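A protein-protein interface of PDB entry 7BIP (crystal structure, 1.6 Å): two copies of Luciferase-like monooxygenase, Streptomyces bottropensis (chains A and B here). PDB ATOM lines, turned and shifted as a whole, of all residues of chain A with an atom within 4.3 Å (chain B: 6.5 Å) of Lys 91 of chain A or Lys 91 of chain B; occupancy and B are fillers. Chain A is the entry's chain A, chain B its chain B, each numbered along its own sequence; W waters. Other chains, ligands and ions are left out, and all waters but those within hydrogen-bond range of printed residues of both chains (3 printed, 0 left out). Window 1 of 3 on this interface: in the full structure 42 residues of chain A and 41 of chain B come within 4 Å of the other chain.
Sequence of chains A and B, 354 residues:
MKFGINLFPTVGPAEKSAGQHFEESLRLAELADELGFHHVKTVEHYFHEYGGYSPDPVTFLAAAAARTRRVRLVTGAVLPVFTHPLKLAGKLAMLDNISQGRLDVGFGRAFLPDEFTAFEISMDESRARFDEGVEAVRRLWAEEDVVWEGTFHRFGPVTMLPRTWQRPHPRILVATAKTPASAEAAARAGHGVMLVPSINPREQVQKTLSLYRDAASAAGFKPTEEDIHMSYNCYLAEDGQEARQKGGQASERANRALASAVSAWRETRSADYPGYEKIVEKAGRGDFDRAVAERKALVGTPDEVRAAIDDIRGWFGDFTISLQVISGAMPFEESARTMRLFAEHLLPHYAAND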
ATOM      1  N   ASP A  56     -18.151 -14.938 -25.646  1.00  0.00           N
ATOM      2  CA  ASP A  56     -19.586 -14.657 -25.747  1.00  0.00           C
ATOM      3  C   ASP A  56     -19.812 -13.170 -25.486  1.00  0.00           C
ATOM      4  O   ASP A  56     -19.975 -12.744 -24.337  1.00  0.00           O
ATOM      5  CB  ASP A  56     -20.386 -15.506 -24.759  1.00  0.00           C
ATOM      6  CG  ASP A  56     -21.859 -15.526 -25.064  1.00  0.00           C
ATOM      7  OD1 ASP A  56     -22.270 -16.253 -25.989  1.00  0.00           O
ATOM      8  OD2 ASP A  56     -22.609 -14.823 -24.371  1.00  0.00           O
ATOM      9  N   VAL A  58     -22.360 -11.311 -25.903  1.00  0.00           N
ATOM     10  CA  VAL A  58     -23.646 -10.992 -25.290  1.00  0.00           C
ATOM     11  C   VAL A  58     -23.538 -11.003 -23.767  1.00  0.00           C
ATOM     12  O   VAL A  58     -24.191 -10.207 -23.088  1.00  0.00           O
ATOM     13  CB  VAL A  58     -24.726 -11.969 -25.796  1.00  0.00           C
ATOM     14  CG1 VAL A  58     -26.016 -11.861 -24.968  1.00  0.00           C
ATOM     15  CG2 VAL A  58     -24.996 -11.710 -27.259  1.00  0.00           C
ATOM     16  N   THR A  59     -22.725 -11.917 -23.202  1.00  0.00           N
ATOM     17  CA  THR A  59     -22.604 -11.997 -21.745  1.00  0.00           C
ATOM     18  C   THR A  59     -21.979 -10.728 -21.181  1.00  0.00           C
ATOM     19  O   THR A  59     -22.474 -10.169 -20.192  1.00  0.00           O
ATOM     20  CB  THR A  59     -21.775 -13.228 -21.343  1.00  0.00           C
ATOM     21  OG1 THR A  59     -22.456 -14.416 -21.764  1.00  0.00           O
ATOM     22  CG2 THR A  59     -21.579 -13.294 -19.821  1.00  0.00           C
ATOM     23  N   LYS A  87     -30.648 -20.091 -30.503  1.00  0.00           N
ATOM     24  CA  LYS A  87     -29.958 -19.568 -29.330  1.00  0.00           C
ATOM     25  C   LYS A  87     -29.510 -18.134 -29.546  1.00  0.00           C
ATOM     26  O   LYS A  87     -29.641 -17.292 -28.647  1.00  0.00           O
ATOM     27  CB  LYS A  87     -28.752 -20.446 -29.036  1.00  0.00           C
ATOM     28  CG  LYS A  87     -29.121 -21.845 -28.671  1.00  0.00           C
ATOM     29  CD  LYS A  87     -29.750 -21.858 -27.326  1.00  0.00           C
ATOM     30  CE  LYS A  87     -28.722 -21.457 -26.296  1.00  0.00           C
ATOM     31  NZ  LYS A  87     -27.513 -22.325 -26.368  1.00  0.00           N
ATOM     32  N   LEU A  88     -28.941 -17.855 -30.719  1.00  0.00           N
ATOM     33  CA  LEU A  88     -28.474 -16.510 -31.017  1.00  0.00           C
ATOM     34  C   LEU A  88     -29.634 -15.525 -31.020  1.00  0.00           C
ATOM     35  O   LEU A  88     -29.556 -14.454 -30.405  1.00  0.00           O
ATOM     36  CB  LEU A  88     -27.751 -16.504 -32.361  1.00  0.00           C
ATOM     37  CG  LEU A  88     -26.979 -15.243 -32.735  1.00  0.00           C
ATOM     38  CD1 LEU A  88     -26.046 -14.804 -31.603  1.00  0.00           C
ATOM     39  CD2 LEU A  88     -26.195 -15.576 -33.989  1.00  0.00           C
ATOM     40  N   ALA A  89     -30.727 -15.870 -31.707  1.00  0.00           N
ATOM     41  CA  ALA A  89     -31.884 -14.980 -31.709  1.00  0.00           C
ATOM     42  C   ALA A  89     -32.414 -14.770 -30.298  1.00  0.00           C
ATOM     43  O   ALA A  89     -32.745 -13.642 -29.912  1.00  0.00           O
ATOM     44  CB  ALA A  89     -32.985 -15.537 -32.609  1.00  0.00           C
ATOM     45  N   GLY A  90     -32.487 -15.850 -29.511  1.00  0.00           N
ATOM     46  CA  GLY A  90     -33.055 -15.747 -28.174  1.00  0.00           C
ATOM     47  C   GLY A  90     -32.220 -14.893 -27.237  1.00  0.00           C
ATOM     48  O   GLY A  90     -32.755 -14.013 -26.558  1.00  0.00           O
ATOM     49  N   LYS A  91     -30.898 -15.141 -27.177  1.00  0.00           N
ATOM     50  CA  LYS A  91     -30.091 -14.363 -26.231  1.00  0.00           C
ATOM     51  C   LYS A  91     -30.016 -12.904 -26.647  1.00  0.00           C
ATOM     52  O   LYS A  91     -30.016 -12.015 -25.786  1.00  0.00           O
ATOM     53  CB  LYS A  91     -28.684 -14.959 -26.068  1.00  0.00           C
ATOM     54  CG  LYS A  91     -27.748 -14.793 -27.260  1.00  0.00           C
ATOM     55  CD  LYS A  91     -26.339 -15.310 -26.920  1.00  0.00           C
ATOM     56  CE  LYS A  91     -26.322 -16.813 -26.751  1.00  0.00           C
ATOM     57  NZ  LYS A  91     -24.916 -17.326 -26.771  1.00  0.00           N
ATOM     58  N   LEU A  92     -30.003 -12.627 -27.951  1.00  0.00           N
ATOM     59  CA  LEU A  92     -29.959 -11.233 -28.384  1.00  0.00           C
ATOM     60  C   LEU A  92     -31.284 -10.529 -28.109  1.00  0.00           C
ATOM     61  O   LEU A  92     -31.299  -9.336 -27.787  1.00  0.00           O
ATOM     62  CB  LEU A  92     -29.609 -11.150 -29.865  1.00  0.00           C
ATOM     63  CG  LEU A  92     -28.156 -11.491 -30.217  1.00  0.00           C
ATOM     64  CD1 LEU A  92     -28.065 -11.696 -31.718  1.00  0.00           C
ATOM     65  CD2 LEU A  92     -27.170 -10.408 -29.730  1.00  0.00           C
ATOM     66  N   ALA A  93     -32.408 -11.248 -28.229  1.00  0.00           N
ATOM     67  CA  ALA A  93     -33.690 -10.656 -27.861  1.00  0.00           C
ATOM     68  C   ALA A  93     -33.755 -10.349 -26.362  1.00  0.00           C
ATOM     69  O   ALA A  93     -34.271  -9.295 -25.958  1.00  0.00           O
ATOM     70  CB  ALA A  93     -34.849 -11.567 -28.298  1.00  0.00           C
ATOM     71  N   MET A  94     -33.213 -11.239 -25.517  1.00  0.00           N
ATOM     72  CA  MET A  94     -33.134 -10.918 -24.092  1.00  0.00           C
ATOM     73  C   MET A  94     -32.326  -9.646 -23.866  1.00  0.00           C
ATOM     74  O   MET A  94     -32.728  -8.758 -23.104  1.00  0.00           O
ATOM     75  CB  MET A  94     -32.513 -12.077 -23.314  1.00  0.00           C
ATOM     76  CG  MET A  94     -33.348 -13.357 -23.250  1.00  0.00           C
ATOM     77  SD  MET A  94     -32.415 -14.615 -22.334  1.00  0.00           S
ATOM     78  CE  MET A  94     -32.536 -14.037 -20.638  1.00  0.00           C
ATOM     79  N   LEU A  95     -31.178  -9.548 -24.526  1.00  0.00           N
ATOM     80  CA  LEU A  95     -30.314  -8.386 -24.338  1.00  0.00           C
ATOM     81  C   LEU A  95     -30.987  -7.105 -24.823  1.00  0.00           C
ATOM     82  O   LEU A  95     -30.861  -6.057 -24.180  1.00  0.00           O
ATOM     83  CB  LEU A  95     -28.988  -8.617 -25.070  1.00  0.00           C
ATOM     84  CG  LEU A  95     -28.036  -7.427 -25.101  1.00  0.00           C
ATOM     85  CD1 LEU A  95     -27.742  -6.961 -23.668  1.00  0.00           C
ATOM     86  CD2 LEU A  95     -26.755  -7.853 -25.815  1.00  0.00           C
ATOM     87  N   PRO B  55     -34.536 -17.889 -22.870  1.00  0.00           N
ATOM     88  CA  PRO B  55     -33.764 -18.904 -23.619  1.00  0.00           C
ATOM     89  C   PRO B  55     -32.286 -18.970 -23.216  1.00  0.00           C
ATOM     90  O   PRO B  55     -31.598 -19.945 -23.566  1.00  0.00           O
ATOM     91  CB  PRO B  55     -33.931 -18.455 -25.079  1.00  0.00           C
ATOM     92  CG  PRO B  55     -34.161 -16.944 -24.978  1.00  0.00           C
ATOM     93  CD  PRO B  55     -34.976 -16.765 -23.716  1.00  0.00           C
ATOM     94  N   ASP B  56     -31.765 -17.970 -22.503  1.00  0.00           N
ATOM     95  CA  ASP B  56     -30.346 -17.943 -22.141  1.00  0.00           C
ATOM     96  C   ASP B  56     -30.202 -17.348 -20.748  1.00  0.00           C
ATOM     97  O   ASP B  56     -30.139 -16.120 -20.580  1.00  0.00           O
ATOM     98  CB  ASP B  56     -29.530 -17.150 -23.166  1.00  0.00           C
ATOM     99  CG  ASP B  56     -28.049 -17.384 -23.030  1.00  0.00           C
ATOM    100  OD1 ASP B  56     -27.586 -18.469 -23.432  1.00  0.00           O
ATOM    101  OD2 ASP B  56     -27.343 -16.488 -22.523  1.00  0.00           O
ATOM    102  N   VAL B  58     -27.717 -17.180 -18.755  1.00  0.00           N
ATOM    103  CA  VAL B  58     -26.468 -16.449 -18.524  1.00  0.00           C
ATOM    104  C   VAL B  58     -26.623 -14.972 -18.890  1.00  0.00           C
ATOM    105  O   VAL B  58     -26.076 -14.088 -18.215  1.00  0.00           O
ATOM    106  CB  VAL B  58     -25.318 -17.127 -19.293  1.00  0.00           C
ATOM    107  CG1 VAL B  58     -24.080 -16.239 -19.337  1.00  0.00           C
ATOM    108  CG2 VAL B  58     -24.980 -18.459 -18.632  1.00  0.00           C
ATOM    109  N   THR B  59     -27.393 -14.674 -19.939  1.00  0.00           N
ATOM    110  CA  THR B  59     -27.597 -13.277 -20.334  1.00  0.00           C
ATOM    111  C   THR B  59     -28.295 -12.481 -19.232  1.00  0.00           C
ATOM    112  O   THR B  59     -27.901 -11.354 -18.909  1.00  0.00           O
ATOM    113  CB  THR B  59     -28.408 -13.224 -21.635  1.00  0.00           C
ATOM    114  OG1 THR B  59     -27.681 -13.908 -22.668  1.00  0.00           O
ATOM    115  CG2 THR B  59     -28.662 -11.791 -22.064  1.00  0.00           C
ATOM    116  N   VAL B  78     -28.730 -24.489 -16.861  1.00  0.00           N
ATOM    117  CA  VAL B  78     -28.295 -24.529 -18.250  1.00  0.00           C
ATOM    118  C   VAL B  78     -28.492 -25.942 -18.765  1.00  0.00           C
ATOM    119  O   VAL B  78     -28.442 -26.918 -18.005  1.00  0.00           O
ATOM    120  CB  VAL B  78     -26.831 -24.079 -18.431  1.00  0.00           C
ATOM    121  CG1 VAL B  78     -26.677 -22.609 -18.076  1.00  0.00           C
ATOM    122  CG2 VAL B  78     -25.879 -24.951 -17.615  1.00  0.00           C
ATOM    123  N   THR B  83     -26.348 -27.049 -26.218  1.00  0.00           N
ATOM    124  CA  THR B  83     -25.224 -26.150 -26.466  1.00  0.00           C
ATOM    125  C   THR B  83     -23.918 -26.933 -26.442  1.00  0.00           C
ATOM    126  O   THR B  83     -23.767 -27.902 -25.696  1.00  0.00           O
ATOM    127  CB  THR B  83     -25.109 -25.014 -25.425  1.00  0.00           C
ATOM    128  OG1 THR B  83     -26.361 -24.335 -25.288  1.00  0.00           O
ATOM    129  CG2 THR B  83     -24.084 -23.981 -25.867  1.00  0.00           C
ATOM    130  N   LEU B  86     -17.847 -26.176 -25.421  1.00  0.00           N
ATOM    131  CA  LEU B  86     -16.924 -25.051 -25.539  1.00  0.00           C
ATOM    132  C   LEU B  86     -17.632 -23.727 -25.292  1.00  0.00           C
ATOM    133  O   LEU B  86     -17.102 -22.855 -24.593  1.00  0.00           O
ATOM    134  CB  LEU B  86     -16.266 -25.042 -26.918  1.00  0.00           C
ATOM    135  CG  LEU B  86     -15.232 -26.151 -27.163  1.00  0.00           C
ATOM    136  CD1 LEU B  86     -14.846 -26.172 -28.637  1.00  0.00           C
ATOM    137  CD2 LEU B  86     -13.996 -25.984 -26.276  1.00  0.00           C
ATOM    138  N   LYS B  87     -18.823 -23.555 -25.867  1.00  0.00           N
ATOM    139  CA  LYS B  87     -19.542 -22.295 -25.694  1.00  0.00           C
ATOM    140  C   LYS B  87     -20.064 -22.152 -24.276  1.00  0.00           C
ATOM    141  O   LYS B  87     -20.005 -21.060 -23.694  1.00  0.00           O
ATOM    142  CB  LYS B  87     -20.695 -22.197 -26.690  1.00  0.00           C
ATOM    143  CG  LYS B  87     -20.250 -22.131 -28.139  1.00  0.00           C
ATOM    144  CD  LYS B  87     -21.446 -21.976 -29.069  1.00  0.00           C
ATOM    145  CE  LYS B  87     -22.072 -20.594 -28.955  1.00  0.00           C
ATOM    146  NZ  LYS B  87     -21.143 -19.533 -29.408  1.00  0.00           N
ATOM    147  N   LEU B  88     -20.593 -23.245 -23.715  1.00  0.00           N
ATOM    148  CA  LEU B  88     -21.107 -23.218 -22.353  1.00  0.00           C
ATOM    149  C   LEU B  88     -20.002 -22.865 -21.359  1.00  0.00           C
ATOM    150  O   LEU B  88     -20.169 -21.970 -20.517  1.00  0.00           O
ATOM    151  CB  LEU B  88     -21.729 -24.576 -22.029  1.00  0.00           C
ATOM    152  CG  LEU B  88     -22.636 -24.683 -20.810  1.00  0.00           C
ATOM    153  CD1 LEU B  88     -23.600 -23.493 -20.754  1.00  0.00           C
ATOM    154  CD2 LEU B  88     -23.389 -26.020 -20.855  1.00  0.00           C
ATOM    155  N   ALA B  89     -18.841 -23.520 -21.478  1.00  0.00           N
ATOM    156  CA  ALA B  89     -17.748 -23.235 -20.549  1.00  0.00           C
ATOM    157  C   ALA B  89     -17.284 -21.786 -20.656  1.00  0.00           C
ATOM    158  O   ALA B  89     -16.996 -21.142 -19.636  1.00  0.00           O
ATOM    159  CB  ALA B  89     -16.571 -24.190 -20.786  1.00  0.00           C
ATOM    160  N   GLY B  90     -17.228 -21.253 -21.878  1.00  0.00           N
ATOM    161  CA  GLY B  90     -16.727 -19.898 -22.064  1.00  0.00           C
ATOM    162  C   GLY B  90     -17.644 -18.831 -21.486  1.00  0.00           C
ATOM    163  O   GLY B  90     -17.192 -17.945 -20.754  1.00  0.00           O
ATOM    164  N   LYS B  91     -18.945 -18.890 -21.811  1.00  0.00           N
ATOM    165  CA  LYS B  91     -19.857 -17.852 -21.333  1.00  0.00           C
ATOM    166  C   LYS B  91     -19.986 -17.906 -19.815  1.00  0.00           C
ATOM    167  O   LYS B  91     -20.089 -16.866 -19.152  1.00  0.00           O
ATOM    168  CB  LYS B  91     -21.223 -17.995 -22.020  1.00  0.00           C
ATOM    169  CG  LYS B  91     -22.049 -19.168 -21.520  1.00  0.00           C
ATOM    170  CD  LYS B  91     -23.190 -19.573 -22.458  1.00  0.00           C
ATOM    171  CE  LYS B  91     -23.879 -18.408 -23.123  1.00  0.00           C
ATOM    172  NZ  LYS B  91     -25.032 -18.909 -23.940  1.00  0.00           N
ATOM    173  N   LEU B  92     -19.949 -19.110 -19.243  1.00  0.00           N
ATOM    174  CA  LEU B  92     -20.040 -19.220 -17.793  1.00  0.00           C
ATOM    175  C   LEU B  92     -18.772 -18.695 -17.130  1.00  0.00           C
ATOM    176  O   LEU B  92     -18.839 -18.059 -16.070  1.00  0.00           O
ATOM    177  CB  LEU B  92     -20.306 -20.671 -17.398  1.00  0.00           C
ATOM    178  CG  LEU B  92     -21.725 -21.137 -17.732  1.00  0.00           C
ATOM    179  CD1 LEU B  92     -21.813 -22.665 -17.677  1.00  0.00           C
ATOM    180  CD2 LEU B  92     -22.722 -20.487 -16.751  1.00  0.00           C
ATOM    181  N   ALA B  93     -17.604 -18.940 -17.743  1.00  0.00           N
ATOM    182  CA  ALA B  93     -16.365 -18.380 -17.200  1.00  0.00           C
ATOM    183  C   ALA B  93     -16.384 -16.854 -17.237  1.00  0.00           C
ATOM    184  O   ALA B  93     -15.915 -16.196 -16.295  1.00  0.00           O
ATOM    185  CB  ALA B  93     -15.154 -18.926 -17.966  1.00  0.00           C
ATOM    186  N   MET B  94     -16.900 -16.271 -18.323  1.00  0.00           N
ATOM    187  CA  MET B  94     -17.096 -14.821 -18.348  1.00  0.00           C
ATOM    188  C   MET B  94     -17.984 -14.380 -17.194  1.00  0.00           C
ATOM    189  O   MET B  94     -17.663 -13.426 -16.476  1.00  0.00           O
ATOM    190  CB  MET B  94     -17.726 -14.377 -19.676  1.00  0.00           C
ATOM    191  CG  MET B  94     -16.868 -14.575 -20.904  1.00  0.00           C
ATOM    192  SD  MET B  94     -17.723 -13.962 -22.388  1.00  0.00           S
ATOM    193  CE  MET B  94     -17.623 -12.180 -22.151  1.00  0.00           C
ATOM    194  N   LEU B  95     -19.128 -15.051 -17.018  1.00  0.00           N
ATOM    195  CA  LEU B  95     -20.050 -14.669 -15.958  1.00  0.00           C
ATOM    196  C   LEU B  95     -19.397 -14.796 -14.583  1.00  0.00           C
ATOM    197  O   LEU B  95     -19.571 -13.924 -13.722  1.00  0.00           O
ATOM    198  CB  LEU B  95     -21.319 -15.520 -16.049  1.00  0.00           C
ATOM    199  CG  LEU B  95     -22.369 -15.290 -14.952  1.00  0.00           C
ATOM    200  CD1 LEU B  95     -22.738 -13.804 -14.829  1.00  0.00           C
ATOM    201  CD2 LEU B  95     -23.607 -16.119 -15.272  1.00  0.00           C
ATOM    202  N   ASP B  96     -18.617 -15.859 -14.373  1.00  0.00           N
ATOM    203  CA  ASP B  96     -17.910 -16.023 -13.103  1.00  0.00           C
ATOM    204  C   ASP B  96     -17.036 -14.812 -12.806  1.00  0.00           C
ATOM    205  O   ASP B  96     -17.029 -14.290 -11.684  1.00  0.00           O
ATOM    206  CB  ASP B  96     -17.053 -17.289 -13.140  1.00  0.00           C
ATOM    207  CG  ASP B  96     -16.529 -17.676 -11.771  1.00  0.00           C
ATOM    208  OD1 ASP B  96     -17.235 -17.368 -10.789  1.00  0.00           O
ATOM    209  OD2 ASP B  96     -15.435 -18.290 -11.688  1.00  0.00           O
ATOM    210  N   ILE B  98     -17.176 -11.698 -14.272  1.00  0.00           N
ATOM    211  CA  ILE B  98     -17.998 -10.493 -14.156  1.00  0.00           C
ATOM    212  C   ILE B  98     -18.585 -10.375 -12.752  1.00  0.00           C
ATOM    213  O   ILE B  98     -18.619  -9.283 -12.161  1.00  0.00           O
ATOM    214  CB  ILE B  98     -19.089 -10.512 -15.247  1.00  0.00           C
ATOM    215  CG1 ILE B  98     -18.456 -10.210 -16.624  1.00  0.00           C
ATOM    216  CG2 ILE B  98     -20.220  -9.539 -14.908  1.00  0.00           C
ATOM    217  CD1 ILE B  98     -19.363 -10.598 -17.800  1.00  0.00           C
ATOM    218  N   LEU B 103     -20.805 -17.025  -8.925  1.00  0.00           N
ATOM    219  CA  LEU B 103     -21.564 -17.960  -9.758  1.00  0.00           C
ATOM    220  C   LEU B 103     -21.577 -19.380  -9.189  1.00  0.00           C
ATOM    221  O   LEU B 103     -20.526 -19.929  -8.849  1.00  0.00           O
ATOM    222  CB  LEU B 103     -20.969 -17.986 -11.165  1.00  0.00           C
ATOM    223  CG  LEU B 103     -21.572 -18.961 -12.177  1.00  0.00           C
ATOM    224  CD1 LEU B 103     -23.036 -18.649 -12.464  1.00  0.00           C
ATOM    225  CD2 LEU B 103     -20.756 -18.907 -13.483  1.00  0.00           C
ATOM    226  N   MET B 160      -9.395 -23.112 -22.378  1.00  0.00           N
ATOM    227  CA  MET B 160     -10.562 -22.256 -22.496  1.00  0.00           C
ATOM    228  C   MET B 160     -10.313 -20.956 -21.744  1.00  0.00           C
ATOM    229  O   MET B 160      -9.892 -20.968 -20.584  1.00  0.00           O
ATOM    230  CB  MET B 160     -11.811 -22.966 -21.960  1.00  0.00           C
ATOM    231  CG  MET B 160     -13.093 -22.082 -21.962  1.00  0.00           C
ATOM    232  SD  MET B 160     -13.575 -21.342 -23.557  1.00  0.00           S
ATOM    233  CE  MET B 160     -13.482 -22.790 -24.584  1.00  0.00           C
ATOM    234  N   LEU B 161     -10.537 -19.839 -22.422  1.00  0.00           N
ATOM    235  CA  LEU B 161     -10.451 -18.512 -21.839  1.00  0.00           C
ATOM    236  C   LEU B 161     -11.847 -17.893 -21.774  1.00  0.00           C
ATOM    237  O   LEU B 161     -12.742 -18.298 -22.516  1.00  0.00           O
ATOM    238  CB  LEU B 161      -9.518 -17.585 -22.634  1.00  0.00           C
ATOM    239  CG  LEU B 161      -8.047 -18.023 -22.711  1.00  0.00           C
ATOM    240  CD1 LEU B 161      -7.235 -17.064 -23.563  1.00  0.00           C
ATOM    241  CD2 LEU B 161      -7.412 -18.195 -21.316  1.00  0.00           C
ATOM    242  N   PRO B 162     -12.097 -16.973 -20.846  1.00  0.00           N
ATOM    243  CA  PRO B 162     -11.196 -16.621 -19.754  1.00  0.00           C
ATOM    244  C   PRO B 162     -11.125 -17.768 -18.762  1.00  0.00           C
ATOM    245  O   PRO B 162     -12.033 -18.605 -18.730  1.00  0.00           O
ATOM    246  CB  PRO B 162     -11.861 -15.388 -19.148  1.00  0.00           C
ATOM    247  CG  PRO B 162     -13.368 -15.641 -19.365  1.00  0.00           C
ATOM    248  CD  PRO B 162     -13.425 -16.334 -20.717  1.00  0.00           C
HETATM  249  O   HOH W   1     -26.211 -21.948 -23.757  1.00  0.00           O
HETATM  250  O   HOH W   2     -20.667 -17.560 -27.665  1.00  0.00           O
HETATM  251  O   HOH W   3     -24.579 -20.163 -26.613  1.00  0.00           O
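NZ of Lys 87 of chain A lies within hydrogen-bond range of OG1 of Thr 83 of chain B.
NZ of Lys 91 of chain B sits close to NZ of Lys 91 of chain A, 3.2 Å away.
SD of Met 94 of chain A sits at hydrogen-bond distance from N of Asp 56 of chain B (3.4 Å).
SD of Met 94 of chain B lies within hydrogen-bond range of N of Asp 56 of chain A, 3.4 Å away.
NZ of Lys 91 of chain B is in salt-bridge range of OD1 of Asp 56 of chain B, 2.6 Å away.
The side-chain hydroxyl of Thr 59 of chain A lies within hydrogen-bond range of the side-chain carboxylate of Asp 56 of chain A.
OD1 of Asp 56 of chain A is in salt-bridge range of NZ of Lys 91 of chain A, at 3.0 Å.
OD2 of Asp 56 of chain B is in hydrogen-bond range of OG1 of Thr 59 of chain B, 2.6 Å away.
Asp 56 of chain A touches Lys 91 of chain B (CB to CB, 3.8 Å).
OG1 of Thr 59 of chain B touches CG1 of Val 58 of chain A, 3.5 Å away.
Val 58 of chain B touches Thr 59 of chain A (CG1 to OG1, 3.4 Å).
CB of Lys 91 of chain B touches OG1 of Thr 59 of chain A, 3.8 Å away.
O of Thr 59 of chain A touches CD1 of Ile 98 of chain B, 3.9 Å away.
Pro 55 of chain B touches Gly 90 of chain A.
Lys 91 of chain A touches Asp 56 of chain B.
OG1 of Thr 59 of chain B touches CB of Lys 91 of chain A (3.7 Å).
Met 94 of chain A touches Pro 55 of chain B (SD to CD, 3.6 Å).
Of chain B, only Asp 56, Thr 59 and Lys 91 come within 4 Å of Lys 91 of chain A.
Lys 91 of chain B touches just these residues of chain A: Asp 56 (3.8 Å), Thr 59 (3.8 Å) and Lys 91 (3.2 Å).
Of the printed residues of chain B, Lys 87 of chain A touches Thr 83 (2.6 Å).
Of the printed residues of chain A, Ile 98 of chain B touches Thr 59.
Of the printed residues of chain B, Val 58 of chain A touches Thr 59 (3.5 Å).
Leu 86 of chain B touches none of the printed residues of chain A.
Leu 92 of chain A touches none of the printed residues of chain B.
The nearest printed residue of chain A that does not touch Lys 91 of chain B is Lys 87 of chain A (4.9 Å).
Printed residues of chain B that touch a printed residue of chain A: Pro 55, Asp 56, Val 58, Thr 59, Thr 83, Lys 91, Met 94 and Ile 98.
Hydrophobic or aromatic side chains of chain B that line the printed part of chain A: Pro 55, Val 58, Met 94 and Ile 98.
Hydrophobic or aromatic side chains of chain A that line the printed part of chain B: Val 58 and Met 94.
Asp 56 of chain A touches Lys 91 of chain B, and with the chains exchanged Lys 91 of chain A touches Asp 56 of chain B.
Asp 56 of chain A touches Met 94 of chain B, and with the chains exchanged Met 94 of chain A touches Asp 56 of chain B.
Thr 59 of chain A touches Lys 91 of chain B, and with the chains exchanged Lys 91 of chain A touches Thr 59 of chain B.
Lys 91 of chain B touches its own counterpart, Lys 91 of chain A.
Water W2 bridges OD1 of Asp 56 of chain A (2.7 Å) and NZ of Lys 87 of chain B (2.7 Å).
Water W1 lies within hydrogen-bond range of OG1 of Thr 83 of chain B (2.8 Å), NZ of Lys 87 of chain A (2.9 Å) and NZ of Lys 91 of chain B (3.3 Å).
Water W3 bridges the side-chain amino group of Lys 91 of chain A (2.9 Å) and the side-chain amino group of Lys 91 of chain B (3.0 Å).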
